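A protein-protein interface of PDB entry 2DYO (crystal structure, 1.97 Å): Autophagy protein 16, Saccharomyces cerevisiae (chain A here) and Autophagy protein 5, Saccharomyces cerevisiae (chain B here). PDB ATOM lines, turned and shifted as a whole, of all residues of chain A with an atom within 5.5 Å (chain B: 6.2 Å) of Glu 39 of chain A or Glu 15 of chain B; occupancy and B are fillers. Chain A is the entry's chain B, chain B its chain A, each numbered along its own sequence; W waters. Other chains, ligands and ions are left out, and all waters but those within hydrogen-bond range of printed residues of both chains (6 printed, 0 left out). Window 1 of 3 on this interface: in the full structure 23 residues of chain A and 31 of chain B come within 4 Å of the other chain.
Printed residues of chain B that touch a printed residue of chain A: Leu 10, Leu 11, Gly 14, Glu 15, Leu 16, Asn 17, Arg 41, Pro 43, Arg 44, Phe 94 and Thr 117. Of the 9 printed residues of chain A, 7 touch a printed residue of chain B. Hydrophobic or aromatic side chains of chain A within 4 Å of the printed part of chain B: Ala 40 and Ile 53. Among the printed residues, 18 pairs touch across the chains. Among the printed residues, Asp or Glu carboxylates within 4 Å of a Lys or Arg side-chain nitrogen of the other chain: Glu 39 of chain A with Arg 44 of chain B (2.6 Å).
The backbone NH (N) of Arg 44 of chain B sits at hydrogen-bond distance from the backbone carbonyl oxygen (O) of Gly 14 of chain B, at 3.2 Å. The backbone carbonyl oxygen (O) of Val 42 of chain B lies within hydrogen-bond range of the backbone NH (N) of Leu 16 of chain B (2.7 Å). The backbone carbonyl oxygen (O) of Thr 117 of chain B is in hydrogen-bond range of the side-chain amide nitrogen (ND2) of Asn 17 of chain B (3.2 Å). NH2 of Arg 44 of chain B is in salt-bridge range of OD1 of Asp 95 of chain B (3.1 Å). The guanidinium group of Arg 35 of chain A lies within hydrogen-bond range of the side-chain amide oxygen of Asn 36 of chain A, at 2.9 Å. The side-chain carboxylate (OE2) of Glu 39 of chain A is in salt-bridge range of the guanidinium group (NE) of Arg 35 of chain A, at 3.996 Å.
Glu 39 of chain A touches six residues of chain B. Glu 15 of chain B touches two residues of chain A. Printed residues of chain B within 4 Å of Arg 35 of chain A: Leu 10 (3.5 Å), Leu 11 (3.8 Å), Gly 14 (3.7 Å) and Arg 44 (3.4 Å). Of the printed residues of chain B, Ile 53 of chain A touches Glu 15 (3.5 Å), Arg 41 (3.5 Å) and Pro 43 (3.7 Å). Of the printed residues of chain B, His 41 of chain A touches Asn 17 (3.2 Å). Printed residues of chain A within 4 Å of Phe 94 of chain B: Glu 39. Asp 95 of chain B touches none of the printed residues of chain A. Val 42 of chain B touches none of the printed residues of chain A.
NH1 of Arg 35 of chain A touches O of Leu 10 of chain B (3.5 Å). Leu 11 of chain B touches Arg 35 of chain A. Arg 35 of chain A touches Gly 14 of chain B. O of Lys 38 of chain A touches OG1 of Thr 117 of chain B (3.98 Å). Glu 15 of chain B touches Glu 39 of chain A (O to CB, 3.5 Å). O of Glu 39 of chain A touches ND2 of Asn 17 of chain B (3.7 Å). Phe 94 of chain B touches Glu 39 of chain A (CE2 to OE1, 3.6 Å). Ala 40 of chain A touches Arg 41 of chain B. Ile 53 of chain A touches Glu 15 of chain B. CD of Pro 43 of chain B touches O of Ile 53 of chain A (3.7 Å).
Water W5 lies within hydrogen-bond range of OE2 of Glu 39 of chain A, OD1 of Asn 36 of chain A and N of Glu 15 of chain B. Water W3 lies within hydrogen-bond range of O of Thr 117 of chain B (2.6 Å), O of Glu 39 of chain A (2.7 Å) and N of Asn 17 of chain B (2.9 Å). Water W4 lies within hydrogen-bond range of O of His 41 of chain A, N of Thr 117 of chain B and O of Lys 38 of chain A. Water W6 lies within hydrogen-bond range of OG1 of Thr 117 of chain B and O of Lys 38 of chain A. Water W1 lies within hydrogen-bond range of the backbone carbonyl oxygen of Asn 36 of chain A (2.8 Å), the backbone carbonyl oxygen of Glu 15 of chain B (2.9 Å), the guanidinium group of Arg 41 of chain B (3.0 Å) and the backbone NH of Ala 40 of chain A (3.1 Å). Water W2 bridges the backbone carbonyl oxygen of Leu 11 of chain B (2.8 Å) and the guanidinium group of Arg 35 of chain A (3.1 Å).
ND2 of Asn 36 of chain A lies within hydrogen-bond range of O of Leu 10 of chain B (2.9 Å). The backbone carbonyl oxygen (O) of His 41 of chain A is in hydrogen-bond range of the side-chain amide nitrogen (ND2) of Asn 17 of chain B (3.2 Å). The guanidinium group (NH1) of Arg 41 of chain B sits at hydrogen-bond distance from the backbone carbonyl oxygen (O) of Glu 39 of chain A, 2.9 Å away. The guanidinium group (NH1) of Arg 44 of chain B is in salt-bridge range of the side-chain carboxylate (OE1) of Glu 39 of chain A (2.6 Å). O of Ile 53 of chain A sits close to O of Arg 41 of chain B (3.5 Å).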
ATOM      1  N   ASP A  34      -2.639  -0.189  11.975  1.00  0.00           N
ATOM      2  CA  ASP A  34      -2.148   1.176  11.862  1.00  0.00           C
ATOM      3  C   ASP A  34      -3.045   2.109  12.652  1.00  0.00           C
ATOM      4  O   ASP A  34      -2.573   3.029  13.319  1.00  0.00           O
ATOM      5  CB  ASP A  34      -2.116   1.601  10.395  1.00  0.00           C
ATOM      6  CG  ASP A  34      -0.805   1.257   9.729  1.00  0.00           C
ATOM      7  OD1 ASP A  34       0.063   2.151   9.644  1.00  0.00           O
ATOM      8  OD2 ASP A  34      -0.635   0.092   9.311  1.00  0.00           O
ATOM      9  N   ARG A  35      -4.347   1.865  12.563  1.00  0.00           N
ATOM     10  CA  ARG A  35      -5.331   2.667  13.278  1.00  0.00           C
ATOM     11  C   ARG A  35      -5.042   2.624  14.779  1.00  0.00           C
ATOM     12  O   ARG A  35      -4.933   3.656  15.431  1.00  0.00           O
ATOM     13  CB  ARG A  35      -6.732   2.106  13.027  1.00  0.00           C
ATOM     14  CG  ARG A  35      -7.843   2.919  13.652  1.00  0.00           C
ATOM     15  CD  ARG A  35      -9.118   2.092  13.774  1.00  0.00           C
ATOM     16  NE  ARG A  35      -8.966   0.996  14.732  1.00  0.00           N
ATOM     17  CZ  ARG A  35      -9.962   0.211  15.129  1.00  0.00           C
ATOM     18  NH1 ARG A  35      -9.738  -0.760  16.011  1.00  0.00           N
ATOM     19  NH2 ARG A  35     -11.184   0.398  14.642  1.00  0.00           N
ATOM     20  N   ASN A  36      -4.931   1.414  15.318  1.00  0.00           N
ATOM     21  CA  ASN A  36      -4.670   1.228  16.741  1.00  0.00           C
ATOM     22  C   ASN A  36      -3.363   1.890  17.176  1.00  0.00           C
ATOM     23  O   ASN A  36      -3.292   2.491  18.251  1.00  0.00           O
ATOM     24  CB  ASN A  36      -4.655  -0.266  17.077  1.00  0.00           C
ATOM     25  CG  ASN A  36      -6.053  -0.878  17.079  1.00  0.00           C
ATOM     26  OD1 ASN A  36      -7.040  -0.188  16.827  1.00  0.00           O
ATOM     27  ND2 ASN A  36      -6.137  -2.172  17.371  1.00  0.00           N
ATOM     28  N   ASP A  37      -2.335   1.786  16.338  1.00  0.00           N
ATOM     29  CA  ASP A  37      -1.041   2.388  16.645  1.00  0.00           C
ATOM     30  C   ASP A  37      -1.184   3.894  16.781  1.00  0.00           C
ATOM     31  O   ASP A  37      -0.768   4.477  17.778  1.00  0.00           O
ATOM     32  CB  ASP A  37      -0.027   2.072  15.542  1.00  0.00           C
ATOM     33  CG  ASP A  37       0.464   0.644  15.593  1.00  0.00           C
ATOM     34  OD1 ASP A  37       1.213   0.239  14.679  1.00  0.00           O
ATOM     35  OD2 ASP A  37       0.107  -0.076  16.550  1.00  0.00           O
ATOM     36  N   LYS A  38      -1.782   4.518  15.769  1.00  0.00           N
ATOM     37  CA  LYS A  38      -1.987   5.961  15.762  1.00  0.00           C
ATOM     38  C   LYS A  38      -2.828   6.427  16.947  1.00  0.00           C
ATOM     39  O   LYS A  38      -2.513   7.433  17.590  1.00  0.00           O
ATOM     40  CB  LYS A  38      -2.653   6.391  14.445  1.00  0.00           C
ATOM     41  N   GLU A  39      -3.900   5.693  17.235  1.00  0.00           N
ATOM     42  CA  GLU A  39      -4.787   6.046  18.336  1.00  0.00           C
ATOM     43  C   GLU A  39      -4.171   5.755  19.707  1.00  0.00           C
ATOM     44  O   GLU A  39      -4.613   6.294  20.721  1.00  0.00           O
ATOM     45  CB  GLU A  39      -6.138   5.332  18.151  1.00  0.00           C
ATOM     46  CG  GLU A  39      -6.925   5.941  16.980  1.00  0.00           C
ATOM     47  CD  GLU A  39      -8.194   5.193  16.591  1.00  0.00           C
ATOM     48  OE1 GLU A  39      -8.887   5.688  15.686  1.00  0.00           O
ATOM     49  OE2 GLU A  39      -8.504   4.130  17.167  1.00  0.00           O
ATOM     50  N   ALA A  40      -3.136   4.923  19.731  1.00  0.00           N
ATOM     51  CA  ALA A  40      -2.461   4.576  20.977  1.00  0.00           C
ATOM     52  C   ALA A  40      -1.318   5.550  21.291  1.00  0.00           C
ATOM     53  O   ALA A  40      -0.800   5.577  22.410  1.00  0.00           O
ATOM     54  CB  ALA A  40      -1.927   3.156  20.893  1.00  0.00           C
ATOM     55  N   HIS A  41      -0.937   6.354  20.304  1.00  0.00           N
ATOM     56  CA  HIS A  41       0.146   7.321  20.475  1.00  0.00           C
ATOM     57  C   HIS A  41      -0.146   8.289  21.622  1.00  0.00           C
ATOM     58  O   HIS A  41      -1.235   8.866  21.707  1.00  0.00           O
ATOM     59  CB  HIS A  41       0.363   8.101  19.173  1.00  0.00           C
ATOM     60  CG  HIS A  41       1.525   9.046  19.223  1.00  0.00           C
ATOM     61  ND1 HIS A  41       1.382  10.410  19.080  1.00  0.00           N
ATOM     62  CD2 HIS A  41       2.844   8.827  19.433  1.00  0.00           C
ATOM     63  CE1 HIS A  41       2.564  10.990  19.202  1.00  0.00           C
ATOM     64  NE2 HIS A  41       3.468  10.051  19.418  1.00  0.00           N
ATOM     65  N   ILE A  53      -9.841   0.032  32.423  1.00  0.00           N
ATOM     66  CA  ILE A  53     -10.026   0.459  31.041  1.00  0.00           C
ATOM     67  C   ILE A  53     -11.495   0.466  30.626  1.00  0.00           C
ATOM     68  O   ILE A  53     -11.989   1.464  30.093  1.00  0.00           O
ATOM     69  CB  ILE A  53      -9.239  -0.457  30.067  1.00  0.00           C
ATOM     70  CG1 ILE A  53      -7.734  -0.289  30.295  1.00  0.00           C
ATOM     71  CG2 ILE A  53      -9.588  -0.118  28.616  1.00  0.00           C
ATOM     72  CD1 ILE A  53      -7.208   1.107  29.994  1.00  0.00           C
ATOM     73  N   LEU B  10      -8.298  -7.126  17.005  1.00  0.00           N
ATOM     74  CA  LEU B  10      -7.817  -5.771  16.776  1.00  0.00           C
ATOM     75  C   LEU B  10      -8.913  -4.759  17.105  1.00  0.00           C
ATOM     76  O   LEU B  10      -8.644  -3.693  17.660  1.00  0.00           O
ATOM     77  CB  LEU B  10      -7.383  -5.596  15.314  1.00  0.00           C
ATOM     78  CG  LEU B  10      -6.077  -6.276  14.893  1.00  0.00           C
ATOM     79  CD1 LEU B  10      -5.860  -6.099  13.394  1.00  0.00           C
ATOM     80  CD2 LEU B  10      -4.917  -5.673  15.674  1.00  0.00           C
ATOM     81  N   LEU B  11     -10.149  -5.096  16.760  1.00  0.00           N
ATOM     82  CA  LEU B  11     -11.279  -4.210  17.026  1.00  0.00           C
ATOM     83  C   LEU B  11     -11.541  -4.156  18.524  1.00  0.00           C
ATOM     84  O   LEU B  11     -11.851  -3.100  19.078  1.00  0.00           O
ATOM     85  CB  LEU B  11     -12.522  -4.714  16.288  1.00  0.00           C
ATOM     86  CG  LEU B  11     -12.386  -4.735  14.757  1.00  0.00           C
ATOM     87  CD1 LEU B  11     -13.668  -5.265  14.120  1.00  0.00           C
ATOM     88  CD2 LEU B  11     -12.090  -3.316  14.257  1.00  0.00           C
ATOM     89  N   TRP B  12     -11.397  -5.303  19.175  1.00  0.00           N
ATOM     90  CA  TRP B  12     -11.616  -5.398  20.613  1.00  0.00           C
ATOM     91  C   TRP B  12     -10.562  -4.578  21.339  1.00  0.00           C
ATOM     92  O   TRP B  12     -10.854  -3.920  22.335  1.00  0.00           O
ATOM     93  CB  TRP B  12     -11.550  -6.859  21.061  1.00  0.00           C
ATOM     94  CG  TRP B  12     -12.049  -7.077  22.453  1.00  0.00           C
ATOM     95  CD1 TRP B  12     -11.305  -7.375  23.559  1.00  0.00           C
ATOM     96  CD2 TRP B  12     -13.414  -7.026  22.889  1.00  0.00           C
ATOM     97  NE1 TRP B  12     -12.123  -7.518  24.658  1.00  0.00           N
ATOM     98  CE2 TRP B  12     -13.423  -7.307  24.275  1.00  0.00           C
ATOM     99  CE3 TRP B  12     -14.631  -6.766  22.243  1.00  0.00           C
ATOM    100  CZ2 TRP B  12     -14.604  -7.341  25.028  1.00  0.00           C
ATOM    101  CZ3 TRP B  12     -15.809  -6.799  22.990  1.00  0.00           C
ATOM    102  CH2 TRP B  12     -15.784  -7.084  24.371  1.00  0.00           C
ATOM    103  N   ASN B  13      -9.334  -4.616  20.831  1.00  0.00           N
ATOM    104  CA  ASN B  13      -8.245  -3.852  21.430  1.00  0.00           C
ATOM    105  C   ASN B  13      -8.312  -2.375  21.016  1.00  0.00           C
ATOM    106  O   ASN B  13      -7.531  -1.551  21.505  1.00  0.00           O
ATOM    107  CB  ASN B  13      -6.893  -4.457  21.033  1.00  0.00           C
ATOM    108  CG  ASN B  13      -6.701  -5.870  21.567  1.00  0.00           C
ATOM    109  OD1 ASN B  13      -5.744  -6.555  21.210  1.00  0.00           O
ATOM    110  ND2 ASN B  13      -7.609  -6.310  22.423  1.00  0.00           N
ATOM    111  N   GLY B  14      -9.245  -2.041  20.123  1.00  0.00           N
ATOM    112  CA  GLY B  14      -9.396  -0.653  19.695  1.00  0.00           C
ATOM    113  C   GLY B  14      -9.524   0.206  20.935  1.00  0.00           C
ATOM    114  O   GLY B  14     -10.200  -0.192  21.885  1.00  0.00           O
ATOM    115  N   GLU B  15      -8.894   1.379  20.944  1.00  0.00           N
ATOM    116  CA  GLU B  15      -8.916   2.233  22.129  1.00  0.00           C
ATOM    117  C   GLU B  15      -8.532   3.677  21.806  1.00  0.00           C
ATOM    118  O   GLU B  15      -7.659   3.926  20.973  1.00  0.00           O
ATOM    119  CB  GLU B  15      -7.945   1.651  23.153  1.00  0.00           C
ATOM    120  CG  GLU B  15      -8.116   2.117  24.579  1.00  0.00           C
ATOM    121  CD  GLU B  15      -7.293   1.262  25.527  1.00  0.00           C
ATOM    122  OE1 GLU B  15      -6.294   1.769  26.075  1.00  0.00           O
ATOM    123  OE2 GLU B  15      -7.637   0.071  25.704  1.00  0.00           O
ATOM    124  N   LEU B  16      -9.171   4.621  22.487  1.00  0.00           N
ATOM    125  CA  LEU B  16      -8.931   6.042  22.257  1.00  0.00           C
ATOM    126  C   LEU B  16      -8.528   6.828  23.498  1.00  0.00           C
ATOM    127  O   LEU B  16      -8.823   6.432  24.625  1.00  0.00           O
ATOM    128  CB  LEU B  16     -10.201   6.689  21.692  1.00  0.00           C
ATOM    129  CG  LEU B  16     -10.732   6.164  20.354  1.00  0.00           C
ATOM    130  CD1 LEU B  16     -12.163   6.666  20.126  1.00  0.00           C
ATOM    131  CD2 LEU B  16      -9.814   6.631  19.235  1.00  0.00           C
ATOM    132  N   ASN B  17      -7.851   7.951  23.274  1.00  0.00           N
ATOM    133  CA  ASN B  17      -7.476   8.845  24.358  1.00  0.00           C
ATOM    134  C   ASN B  17      -8.716   9.724  24.481  1.00  0.00           C
ATOM    135  O   ASN B  17      -9.182  10.282  23.488  1.00  0.00           O
ATOM    136  CB  ASN B  17      -6.270   9.721  23.980  1.00  0.00           C
ATOM    137  CG  ASN B  17      -4.984   8.931  23.848  1.00  0.00           C
ATOM    138  OD1 ASN B  17      -4.686   8.060  24.667  1.00  0.00           O
ATOM    139  ND2 ASN B  17      -4.198   9.248  22.825  1.00  0.00           N
ATOM    140  N   ARG B  41      -8.397   6.148  28.952  1.00  0.00           N
ATOM    141  CA  ARG B  41      -8.320   5.340  27.749  1.00  0.00           C
ATOM    142  C   ARG B  41      -9.666   4.641  27.687  1.00  0.00           C
ATOM    143  O   ARG B  41     -10.098   4.014  28.660  1.00  0.00           O
ATOM    144  CB  ARG B  41      -7.182   4.322  27.851  1.00  0.00           C
ATOM    145  CG  ARG B  41      -5.807   4.952  27.673  1.00  0.00           C
ATOM    146  CD  ARG B  41      -5.599   5.393  26.225  1.00  0.00           C
ATOM    147  NE  ARG B  41      -5.302   4.265  25.345  1.00  0.00           N
ATOM    148  CZ  ARG B  41      -5.152   4.367  24.027  1.00  0.00           C
ATOM    149  NH1 ARG B  41      -5.278   5.544  23.435  1.00  0.00           N
ATOM    150  NH2 ARG B  41      -4.871   3.296  23.300  1.00  0.00           N
ATOM    151  N   VAL B  42     -10.335   4.769  26.547  1.00  0.00           N
ATOM    152  CA  VAL B  42     -11.655   4.188  26.359  1.00  0.00           C
ATOM    153  C   VAL B  42     -11.699   3.324  25.106  1.00  0.00           C
ATOM    154  O   VAL B  42     -11.264   3.756  24.035  1.00  0.00           O
ATOM    155  CB  VAL B  42     -12.710   5.304  26.215  1.00  0.00           C
ATOM    156  CG1 VAL B  42     -14.076   4.709  25.917  1.00  0.00           C
ATOM    157  CG2 VAL B  42     -12.751   6.145  27.485  1.00  0.00           C
ATOM    158  N   PRO B  43     -12.215   2.090  25.226  1.00  0.00           N
ATOM    159  CA  PRO B  43     -12.294   1.209  24.061  1.00  0.00           C
ATOM    160  C   PRO B  43     -13.207   1.818  22.996  1.00  0.00           C
ATOM    161  O   PRO B  43     -14.111   2.600  23.310  1.00  0.00           O
ATOM    162  CB  PRO B  43     -12.898  -0.078  24.634  1.00  0.00           C
ATOM    163  CG  PRO B  43     -12.442  -0.066  26.075  1.00  0.00           C
ATOM    164  CD  PRO B  43     -12.634   1.385  26.453  1.00  0.00           C
ATOM    165  N   ARG B  44     -12.959   1.481  21.737  1.00  0.00           N
ATOM    166  CA  ARG B  44     -13.823   1.960  20.671  1.00  0.00           C
ATOM    167  C   ARG B  44     -15.142   1.201  20.838  1.00  0.00           C
ATOM    168  O   ARG B  44     -16.220   1.732  20.588  1.00  0.00           O
ATOM    169  CB  ARG B  44     -13.216   1.642  19.301  1.00  0.00           C
ATOM    170  CG  ARG B  44     -12.388   2.777  18.697  1.00  0.00           C
ATOM    171  CD  ARG B  44     -11.726   2.316  17.404  1.00  0.00           C
ATOM    172  NE  ARG B  44     -11.206   3.420  16.603  1.00  0.00           N
ATOM    173  CZ  ARG B  44     -11.913   4.076  15.689  1.00  0.00           C
ATOM    174  NH1 ARG B  44     -11.359   5.068  15.006  1.00  0.00           N
ATOM    175  NH2 ARG B  44     -13.178   3.739  15.454  1.00  0.00           N
ATOM    176  N   PHE B  94     -16.562   8.608  17.336  1.00  0.00           N
ATOM    177  CA  PHE B  94     -15.268   9.143  16.921  1.00  0.00           C
ATOM    178  C   PHE B  94     -15.185   9.287  15.403  1.00  0.00           C
ATOM    179  O   PHE B  94     -14.772  10.330  14.896  1.00  0.00           O
ATOM    180  CB  PHE B  94     -14.131   8.231  17.396  1.00  0.00           C
ATOM    181  CG  PHE B  94     -12.758   8.756  17.063  1.00  0.00           C
ATOM    182  CD1 PHE B  94     -12.173   9.752  17.834  1.00  0.00           C
ATOM    183  CD2 PHE B  94     -12.060   8.261  15.968  1.00  0.00           C
ATOM    184  CE1 PHE B  94     -10.903  10.251  17.519  1.00  0.00           C
ATOM    185  CE2 PHE B  94     -10.794   8.752  15.642  1.00  0.00           C
ATOM    186  CZ  PHE B  94     -10.214   9.746  16.422  1.00  0.00           C
ATOM    187  N   ASP B  95     -15.560   8.232  14.683  1.00  0.00           N
ATOM    188  CA  ASP B  95     -15.515   8.253  13.224  1.00  0.00           C
ATOM    189  C   ASP B  95     -16.371   9.381  12.676  1.00  0.00           C
ATOM    190  O   ASP B  95     -15.999  10.044  11.709  1.00  0.00           O
ATOM    191  CB  ASP B  95     -16.004   6.922  12.643  1.00  0.00           C
ATOM    192  CG  ASP B  95     -15.042   5.783  12.897  1.00  0.00           C
ATOM    193  OD1 ASP B  95     -13.967   6.030  13.476  1.00  0.00           O
ATOM    194  OD2 ASP B  95     -15.356   4.637  12.509  1.00  0.00           O
ATOM    195  N   THR B 117      -4.165  12.295  18.862  1.00  0.00           N
ATOM    196  CA  THR B 117      -5.475  11.793  18.481  1.00  0.00           C
ATOM    197  C   THR B 117      -6.248  11.569  19.773  1.00  0.00           C
ATOM    198  O   THR B 117      -5.905  10.693  20.561  1.00  0.00           O
ATOM    199  CB  THR B 117      -5.381  10.458  17.723  1.00  0.00           C
ATOM    200  OG1 THR B 117      -4.618  10.637  16.523  1.00  0.00           O
ATOM    201  CG2 THR B 117      -6.774   9.962  17.354  1.00  0.00           C
ATOM    202  N   GLY B 257     -13.123   3.201  11.787  1.00  0.00           N
ATOM    203  CA  GLY B 257     -12.006   4.112  11.620  1.00  0.00           C
ATOM    204  C   GLY B 257     -11.093   3.933  10.424  1.00  0.00           C
ATOM    205  O   GLY B 257     -10.071   4.618  10.340  1.00  0.00           O
HETATM  206  O   HOH W   1      -5.115   2.592  20.371  1.00  0.00           O
HETATM  207  O   HOH W   2     -12.574  -1.140  17.169  1.00  0.00           O
HETATM  208  O   HOH W   3      -6.543   8.154  20.638  1.00  0.00           O
HETATM  209  O   HOH W   4      -2.569  10.050  19.773  1.00  0.00           O
HETATM  210  O   HOH W   5      -7.636   2.035  18.431  1.00  0.00           O
HETATM  211  O   HOH W   6      -2.035  10.085  16.729  1.00  0.00           O
